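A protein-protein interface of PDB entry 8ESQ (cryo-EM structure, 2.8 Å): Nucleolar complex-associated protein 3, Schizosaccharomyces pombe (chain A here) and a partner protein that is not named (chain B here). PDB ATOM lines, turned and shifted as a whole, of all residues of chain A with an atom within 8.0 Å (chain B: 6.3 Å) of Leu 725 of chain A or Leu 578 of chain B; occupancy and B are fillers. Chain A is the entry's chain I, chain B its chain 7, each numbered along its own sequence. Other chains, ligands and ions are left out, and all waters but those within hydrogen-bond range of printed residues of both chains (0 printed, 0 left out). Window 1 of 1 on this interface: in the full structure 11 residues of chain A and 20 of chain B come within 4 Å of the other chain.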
ATOM      1  N   PHE A 595      33.068  25.436  25.187  1.00  0.00           N
ATOM      2  CA  PHE A 595      32.804  24.635  26.382  1.00  0.00           C
ATOM      3  C   PHE A 595      33.241  25.317  27.673  1.00  0.00           C
ATOM      4  O   PHE A 595      32.433  25.367  28.617  1.00  0.00           O
ATOM      5  CB  PHE A 595      33.445  23.251  26.227  1.00  0.00           C
ATOM      6  CG  PHE A 595      32.607  22.282  25.451  1.00  0.00           C
ATOM      7  CD1 PHE A 595      32.537  22.353  24.072  1.00  0.00           C
ATOM      8  CD2 PHE A 595      31.893  21.291  26.104  1.00  0.00           C
ATOM      9  CE1 PHE A 595      31.763  21.460  23.358  1.00  0.00           C
ATOM     10  CE2 PHE A 595      31.120  20.393  25.394  1.00  0.00           C
ATOM     11  CZ  PHE A 595      31.055  20.478  24.020  1.00  0.00           C
ATOM     12  N   ALA A 660      24.566  24.608  20.617  1.00  0.00           N
ATOM     13  CA  ALA A 660      23.384  24.235  21.387  1.00  0.00           C
ATOM     14  C   ALA A 660      23.770  23.616  22.725  1.00  0.00           C
ATOM     15  O   ALA A 660      23.120  23.870  23.745  1.00  0.00           O
ATOM     16  CB  ALA A 660      22.512  23.273  20.580  1.00  0.00           C
ATOM     17  N   ILE A 661      24.821  22.792  22.738  1.00  0.00           N
ATOM     18  CA  ILE A 661      25.285  22.194  23.989  1.00  0.00           C
ATOM     19  C   ILE A 661      25.742  23.279  24.956  1.00  0.00           C
ATOM     20  O   ILE A 661      25.433  23.239  26.153  1.00  0.00           O
ATOM     21  CB  ILE A 661      26.404  21.172  23.717  1.00  0.00           C
ATOM     22  CG1 ILE A 661      25.954  20.147  22.675  1.00  0.00           C
ATOM     23  CG2 ILE A 661      26.819  20.480  25.007  1.00  0.00           C
ATOM     24  CD1 ILE A 661      27.020  19.139  22.309  1.00  0.00           C
ATOM     25  N   MET A 664      23.122  25.442  27.225  1.00  0.00           N
ATOM     26  CA  MET A 664      22.380  24.860  28.339  1.00  0.00           C
ATOM     27  C   MET A 664      22.174  25.872  29.463  1.00  0.00           C
ATOM     28  O   MET A 664      21.187  25.791  30.205  1.00  0.00           O
ATOM     29  CB  MET A 664      23.091  23.593  28.829  1.00  0.00           C
ATOM     30  CG  MET A 664      24.346  23.782  29.684  1.00  0.00           C
ATOM     31  SD  MET A 664      24.070  24.292  31.394  1.00  0.00           S
ATOM     32  CE  MET A 664      24.314  22.743  32.254  1.00  0.00           C
ATOM     33  N   TYR A 721      17.569  16.954  20.378  1.00  0.00           N
ATOM     34  CA  TYR A 721      17.764  16.383  21.706  1.00  0.00           C
ATOM     35  C   TYR A 721      17.820  17.470  22.774  1.00  0.00           C
ATOM     36  O   TYR A 721      17.095  17.414  23.767  1.00  0.00           O
ATOM     37  CB  TYR A 721      19.043  15.545  21.746  1.00  0.00           C
ATOM     38  CG  TYR A 721      18.925  14.204  21.059  1.00  0.00           C
ATOM     39  CD1 TYR A 721      18.351  13.118  21.706  1.00  0.00           C
ATOM     40  CD2 TYR A 721      19.388  14.023  19.763  1.00  0.00           C
ATOM     41  CE1 TYR A 721      18.240  11.890  21.083  1.00  0.00           C
ATOM     42  CE2 TYR A 721      19.282  12.799  19.130  1.00  0.00           C
ATOM     43  CZ  TYR A 721      18.707  11.737  19.796  1.00  0.00           C
ATOM     44  OH  TYR A 721      18.599  10.515  19.170  1.00  0.00           O
ATOM     45  N   GLU A 722      18.694  18.451  22.560  1.00  0.00           N
ATOM     46  CA  GLU A 722      18.858  19.527  23.534  1.00  0.00           C
ATOM     47  C   GLU A 722      17.578  20.310  23.816  1.00  0.00           C
ATOM     48  O   GLU A 722      17.322  20.599  24.999  1.00  0.00           O
ATOM     49  CB  GLU A 722      19.980  20.468  23.079  1.00  0.00           C
ATOM     50  CG  GLU A 722      20.321  21.562  24.081  1.00  0.00           C
ATOM     51  CD  GLU A 722      20.887  21.019  25.380  1.00  0.00           C
ATOM     52  OE1 GLU A 722      21.477  19.917  25.363  1.00  0.00           O
ATOM     53  OE2 GLU A 722      20.744  21.696  26.420  1.00  0.00           O
ATOM     54  N   PRO A 723      16.754  20.692  22.829  1.00  0.00           N
ATOM     55  CA  PRO A 723      15.545  21.466  23.161  1.00  0.00           C
ATOM     56  C   PRO A 723      14.611  20.765  24.130  1.00  0.00           C
ATOM     57  O   PRO A 723      13.908  21.443  24.888  1.00  0.00           O
ATOM     58  CB  PRO A 723      14.877  21.677  21.796  1.00  0.00           C
ATOM     59  CG  PRO A 723      15.976  21.595  20.823  1.00  0.00           C
ATOM     60  CD  PRO A 723      16.943  20.589  21.370  1.00  0.00           C
ATOM     61  N   PHE A 724      14.578  19.429  24.126  1.00  0.00           N
ATOM     62  CA  PHE A 724      13.691  18.711  25.038  1.00  0.00           C
ATOM     63  C   PHE A 724      14.024  19.024  26.491  1.00  0.00           C
ATOM     64  O   PHE A 724      13.123  19.262  27.305  1.00  0.00           O
ATOM     65  CB  PHE A 724      13.774  17.207  24.777  1.00  0.00           C
ATOM     66  CG  PHE A 724      13.518  16.822  23.347  1.00  0.00           C
ATOM     67  CD1 PHE A 724      12.598  17.517  22.581  1.00  0.00           C
ATOM     68  CD2 PHE A 724      14.200  15.763  22.771  1.00  0.00           C
ATOM     69  CE1 PHE A 724      12.361  17.165  21.266  1.00  0.00           C
ATOM     70  CE2 PHE A 724      13.968  15.406  21.455  1.00  0.00           C
ATOM     71  CZ  PHE A 724      13.047  16.108  20.703  1.00  0.00           C
ATOM     72  N   LEU A 725      15.311  19.028  26.838  1.00  0.00           N
ATOM     73  CA  LEU A 725      15.713  19.418  28.184  1.00  0.00           C
ATOM     74  C   LEU A 725      15.642  20.927  28.382  1.00  0.00           C
ATOM     75  O   LEU A 725      15.431  21.391  29.508  1.00  0.00           O
ATOM     76  CB  LEU A 725      17.124  18.908  28.479  1.00  0.00           C
ATOM     77  CG  LEU A 725      17.599  19.015  29.930  1.00  0.00           C
ATOM     78  CD1 LEU A 725      16.690  18.216  30.850  1.00  0.00           C
ATOM     79  CD2 LEU A 725      19.039  18.545  30.058  1.00  0.00           C
ATOM     80  N   LEU A 726      15.815  21.704  27.309  1.00  0.00           N
ATOM     81  CA  LEU A 726      15.751  23.158  27.425  1.00  0.00           C
ATOM     82  C   LEU A 726      14.352  23.635  27.794  1.00  0.00           C
ATOM     83  O   LEU A 726      14.205  24.692  28.419  1.00  0.00           O
ATOM     84  CB  LEU A 726      16.205  23.813  26.121  1.00  0.00           C
ATOM     85  CG  LEU A 726      17.697  23.732  25.792  1.00  0.00           C
ATOM     86  CD1 LEU A 726      17.981  24.368  24.441  1.00  0.00           C
ATOM     87  CD2 LEU A 726      18.529  24.386  26.885  1.00  0.00           C
ATOM     88  N   LYS A 727      13.319  22.883  27.408  1.00  0.00           N
ATOM     89  CA  LYS A 727      11.953  23.246  27.775  1.00  0.00           C
ATOM     90  C   LYS A 727      11.802  23.348  29.285  1.00  0.00           C
ATOM     91  O   LYS A 727      11.150  24.267  29.795  1.00  0.00           O
ATOM     92  CB  LYS A 727      10.971  22.218  27.208  1.00  0.00           C
ATOM     93  CG  LYS A 727      10.969  22.136  25.694  1.00  0.00           C
ATOM     94  CD  LYS A 727      10.155  20.954  25.198  1.00  0.00           C
ATOM     95  CE  LYS A 727      10.162  20.881  23.681  1.00  0.00           C
ATOM     96  NZ  LYS A 727      11.505  20.529  23.146  1.00  0.00           N
ATOM     97  N   ASN A 728      12.401  22.415  30.017  1.00  0.00           N
ATOM     98  CA  ASN A 728      12.389  22.434  31.476  1.00  0.00           C
ATOM     99  C   ASN A 728      13.558  23.285  31.956  1.00  0.00           C
ATOM    100  O   ASN A 728      14.684  22.801  32.077  1.00  0.00           O
ATOM    101  CB  ASN A 728      12.472  21.014  32.023  1.00  0.00           C
ATOM    102  CG  ASN A 728      11.311  20.150  31.578  1.00  0.00           C
ATOM    103  OD1 ASN A 728      11.487  19.194  30.824  1.00  0.00           O
ATOM    104  ND2 ASN A 728      10.115  20.483  32.046  1.00  0.00           N
ATOM    105  N   HIS A 729      13.298  24.564  32.224  1.00  0.00           N
ATOM    106  CA  HIS A 729      14.354  25.455  32.677  1.00  0.00           C
ATOM    107  C   HIS A 729      13.711  26.588  33.469  1.00  0.00           C
ATOM    108  O   HIS A 729      12.506  26.832  33.366  1.00  0.00           O
ATOM    109  CB  HIS A 729      15.195  25.952  31.484  1.00  0.00           C
ATOM    110  CG  HIS A 729      15.786  27.316  31.662  1.00  0.00           C
ATOM    111  ND1 HIS A 729      15.046  28.476  31.579  1.00  0.00           N
ATOM    112  CD2 HIS A 729      17.061  27.701  31.911  1.00  0.00           C
ATOM    113  CE1 HIS A 729      15.837  29.515  31.777  1.00  0.00           C
ATOM    114  NE2 HIS A 729      17.064  29.073  31.978  1.00  0.00           N
ATOM    115  N   TYR A 730      14.537  27.275  34.267  1.00  0.00           N
ATOM    116  CA  TYR A 730      14.032  28.208  35.274  1.00  0.00           C
ATOM    117  C   TYR A 730      13.090  29.250  34.678  1.00  0.00           C
ATOM    118  O   TYR A 730      11.972  29.439  35.173  1.00  0.00           O
ATOM    119  CB  TYR A 730      15.206  28.896  35.970  1.00  0.00           C
ATOM    120  CG  TYR A 730      15.852  28.060  37.050  1.00  0.00           C
ATOM    121  CD1 TYR A 730      15.143  27.055  37.695  1.00  0.00           C
ATOM    122  CD2 TYR A 730      17.173  28.271  37.418  1.00  0.00           C
ATOM    123  CE1 TYR A 730      15.731  26.286  38.679  1.00  0.00           C
ATOM    124  CE2 TYR A 730      17.771  27.505  38.401  1.00  0.00           C
ATOM    125  CZ  TYR A 730      17.044  26.516  39.029  1.00  0.00           C
ATOM    126  OH  TYR A 730      17.629  25.751  40.011  1.00  0.00           O
ATOM    127  N   VAL A 734      11.779  30.073  28.064  1.00  0.00           N
ATOM    128  CA  VAL A 734      12.643  29.160  27.320  1.00  0.00           C
ATOM    129  C   VAL A 734      11.827  28.007  26.751  1.00  0.00           C
ATOM    130  O   VAL A 734      12.123  27.491  25.665  1.00  0.00           O
ATOM    131  CB  VAL A 734      13.797  28.671  28.212  1.00  0.00           C
ATOM    132  CG1 VAL A 734      14.696  27.712  27.449  1.00  0.00           C
ATOM    133  CG2 VAL A 734      14.593  29.859  28.697  1.00  0.00           C
ATOM    134  N   SER A 735      10.788  27.583  27.476  1.00  0.00           N
ATOM    135  CA  SER A 735       9.913  26.528  26.976  1.00  0.00           C
ATOM    136  C   SER A 735       9.271  26.922  25.652  1.00  0.00           C
ATOM    137  O   SER A 735       9.320  26.160  24.680  1.00  0.00           O
ATOM    138  CB  SER A 735       8.838  26.202  28.014  1.00  0.00           C
ATOM    139  OG  SER A 735       9.377  25.492  29.114  1.00  0.00           O
ATOM    140  N   ALA A 738      11.797  27.014  22.889  1.00  0.00           N
ATOM    141  CA  ALA A 738      12.020  25.678  22.348  1.00  0.00           C
ATOM    142  C   ALA A 738      10.858  25.241  21.466  1.00  0.00           C
ATOM    143  O   ALA A 738      11.065  24.609  20.423  1.00  0.00           O
ATOM    144  CB  ALA A 738      12.242  24.681  23.484  1.00  0.00           C
ATOM    145  N   PHE B 504      14.640  21.401  34.651  1.00  0.00           N
ATOM    146  CA  PHE B 504      16.076  21.219  34.797  1.00  0.00           C
ATOM    147  C   PHE B 504      16.727  22.491  35.326  1.00  0.00           C
ATOM    148  O   PHE B 504      16.258  23.607  35.083  1.00  0.00           O
ATOM    149  CB  PHE B 504      16.707  20.822  33.463  1.00  0.00           C
ATOM    150  N   ALA B 508      25.098  22.619  37.229  1.00  0.00           N
ATOM    151  CA  ALA B 508      26.358  21.975  36.868  1.00  0.00           C
ATOM    152  C   ALA B 508      27.526  22.948  36.873  1.00  0.00           C
ATOM    153  O   ALA B 508      28.591  22.598  37.411  1.00  0.00           O
ATOM    154  CB  ALA B 508      26.212  21.289  35.505  1.00  0.00           C
ATOM    155  N   TYR B 569      18.417  14.480  35.866  1.00  0.00           N
ATOM    156  CA  TYR B 569      18.478  14.715  34.431  1.00  0.00           C
ATOM    157  C   TYR B 569      18.696  13.439  33.627  1.00  0.00           C
ATOM    158  O   TYR B 569      18.799  13.510  32.399  1.00  0.00           O
ATOM    159  CB  TYR B 569      19.589  15.720  34.109  1.00  0.00           C
ATOM    160  N   ASP B 572      16.122  12.572  30.869  1.00  0.00           N
ATOM    161  CA  ASP B 572      16.118  13.389  29.663  1.00  0.00           C
ATOM    162  C   ASP B 572      16.727  12.631  28.490  1.00  0.00           C
ATOM    163  O   ASP B 572      17.669  11.852  28.652  1.00  0.00           O
ATOM    164  CB  ASP B 572      16.887  14.689  29.904  1.00  0.00           C
ATOM    165  N   ILE B 573      16.168  12.859  27.299  1.00  0.00           N
ATOM    166  CA  ILE B 573      16.683  12.212  26.095  1.00  0.00           C
ATOM    167  C   ILE B 573      18.109  12.665  25.816  1.00  0.00           C
ATOM    168  O   ILE B 573      18.969  11.862  25.431  1.00  0.00           O
ATOM    169  CB  ILE B 573      15.756  12.491  24.898  1.00  0.00           C
ATOM    170  N   SER B 574      18.385  13.956  26.002  1.00  0.00           N
ATOM    171  CA  SER B 574      19.706  14.521  25.774  1.00  0.00           C
ATOM    172  C   SER B 574      20.602  14.443  27.006  1.00  0.00           C
ATOM    173  O   SER B 574      21.530  15.249  27.133  1.00  0.00           O
ATOM    174  CB  SER B 574      19.585  15.974  25.311  1.00  0.00           C
ATOM    175  N   PHE B 575      20.336  13.505  27.914  1.00  0.00           N
ATOM    176  CA  PHE B 575      21.155  13.363  29.117  1.00  0.00           C
ATOM    177  C   PHE B 575      22.631  13.161  28.811  1.00  0.00           C
ATOM    178  O   PHE B 575      23.465  13.829  29.441  1.00  0.00           O
ATOM    179  CB  PHE B 575      20.612  12.205  29.967  1.00  0.00           C
ATOM    180  N   PRO B 576      23.023  12.274  27.892  1.00  0.00           N
ATOM    181  CA  PRO B 576      24.446  12.193  27.529  1.00  0.00           C
ATOM    182  C   PRO B 576      24.990  13.480  26.937  1.00  0.00           C
ATOM    183  O   PRO B 576      26.159  13.813  27.168  1.00  0.00           O
ATOM    184  CB  PRO B 576      24.480  11.043  26.513  1.00  0.00           C
ATOM    185  N   GLU B 577      24.175  14.217  26.179  1.00  0.00           N
ATOM    186  CA  GLU B 577      24.648  15.454  25.566  1.00  0.00           C
ATOM    187  C   GLU B 577      24.847  16.550  26.605  1.00  0.00           C
ATOM    188  O   GLU B 577      25.845  17.280  26.562  1.00  0.00           O
ATOM    189  CB  GLU B 577      23.670  15.910  24.484  1.00  0.00           C
ATOM    190  N   LEU B 578      23.907  16.685  27.544  1.00  0.00           N
ATOM    191  CA  LEU B 578      24.010  17.741  28.547  1.00  0.00           C
ATOM    192  C   LEU B 578      25.150  17.486  29.523  1.00  0.00           C
ATOM    193  O   LEU B 578      25.723  18.438  30.065  1.00  0.00           O
ATOM    194  CB  LEU B 578      22.688  17.878  29.301  1.00  0.00           C
ATOM    195  N   VAL B 579      25.495  16.217  29.763  1.00  0.00           N
ATOM    196  CA  VAL B 579      26.559  15.885  30.706  1.00  0.00           C
ATOM    197  C   VAL B 579      27.928  15.794  30.046  1.00  0.00           C
ATOM    198  O   VAL B 579      28.933  15.624  30.755  1.00  0.00           O
ATOM    199  CB  VAL B 579      26.261  14.559  31.431  1.00  0.00           C
ATOM    200  N   ILE B 580      28.003  15.891  28.716  1.00  0.00           N
ATOM    201  CA  ILE B 580      29.299  15.821  28.040  1.00  0.00           C
ATOM    202  C   ILE B 580      30.222  16.953  28.475  1.00  0.00           C
ATOM    203  O   ILE B 580      31.393  16.682  28.785  1.00  0.00           O
ATOM    204  CB  ILE B 580      29.097  15.779  26.516  1.00  0.00           C
ATOM    205  N   PRO B 581      29.787  18.217  28.506  1.00  0.00           N
ATOM    206  CA  PRO B 581      30.689  19.279  28.985  1.00  0.00           C
ATOM    207  C   PRO B 581      31.167  19.065  30.410  1.00  0.00           C
ATOM    208  O   PRO B 581      32.330  19.355  30.721  1.00  0.00           O
ATOM    209  CB  PRO B 581      29.832  20.545  28.854  1.00  0.00           C
ATOM    210  N   ALA B 582      30.298  18.562  31.288  1.00  0.00           N
ATOM    211  CA  ALA B 582      30.709  18.295  32.662  1.00  0.00           C
ATOM    212  C   ALA B 582      31.701  17.142  32.727  1.00  0.00           C
ATOM    213  O   ALA B 582      32.653  17.175  33.515  1.00  0.00           O
ATOM    214  CB  ALA B 582      29.485  18.001  33.529  1.00  0.00           C
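The backbone NH (N) of Phe 504 of chain B lies within hydrogen-bond range of the backbone carbonyl oxygen (O) of Asn 728 of chain A (2.9 Å).
Hydrophobic or aromatic side chains of chain A that line the printed part of chain B: Phe 595, Ile 661, Tyr 721 and Leu 725. Along chain A the printed residues that touch a printed residue of chain B span positions 595 to 729.
Of the printed residues of chain B, Phe 595 of chain A touches Pro 581 (3.5 Å). Leu 725 of chain A touches three residues of chain B. Of the printed residues of chain B, Asn 728 of chain A touches Phe 504 (2.9 Å). Printed residues of chain B within 4 Å of His 729 of chain A: Phe 504. Of the printed residues of chain A, Phe 504 of chain B touches Leu 725 (3.7 Å), Asn 728 (2.9 Å) and His 729 (3.6 Å). Printed residues of chain A within 4 Å of Leu 578 of chain B: Leu 725 (3.8 Å). Val 579 of chain B touches none of the printed residues of chain A. The nearest printed residue of chain B that does not touch Leu 725 of chain A is Tyr 569 of chain B (5.0 Å). The nearest residue of chain A that does not touch Leu 578 of chain B is Glu 722 of chain A (4.6 Å). The nearest printed residue of chain A that does not touch Pro 581 of chain B is Ile 661 of chain A (4.9 Å).
Among the printed residues, pairs that only touch across the chains: Tyr 721 of chain A with Ser 574 of chain B (3.3 Å), Phe 595 of chain A with Pro 581 of chain B (3.5 Å), His 729 of chain A with Phe 504 of chain B (3.6 Å), Leu 725 of chain A with Asp 572 of chain B (3.7 Å), Ile 661 of chain A with Glu 577 of chain B (3.7 Å), Leu 725 of chain A with Phe 504 of chain B (3.7 Å), Leu 725 of chain A with Leu 578 of chain B (3.8 Å), Glu 722 of chain A with Ser 574 of chain B (3.8 Å) and Tyr 721 of chain A with Ile 573 of chain B (3.98 Å).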
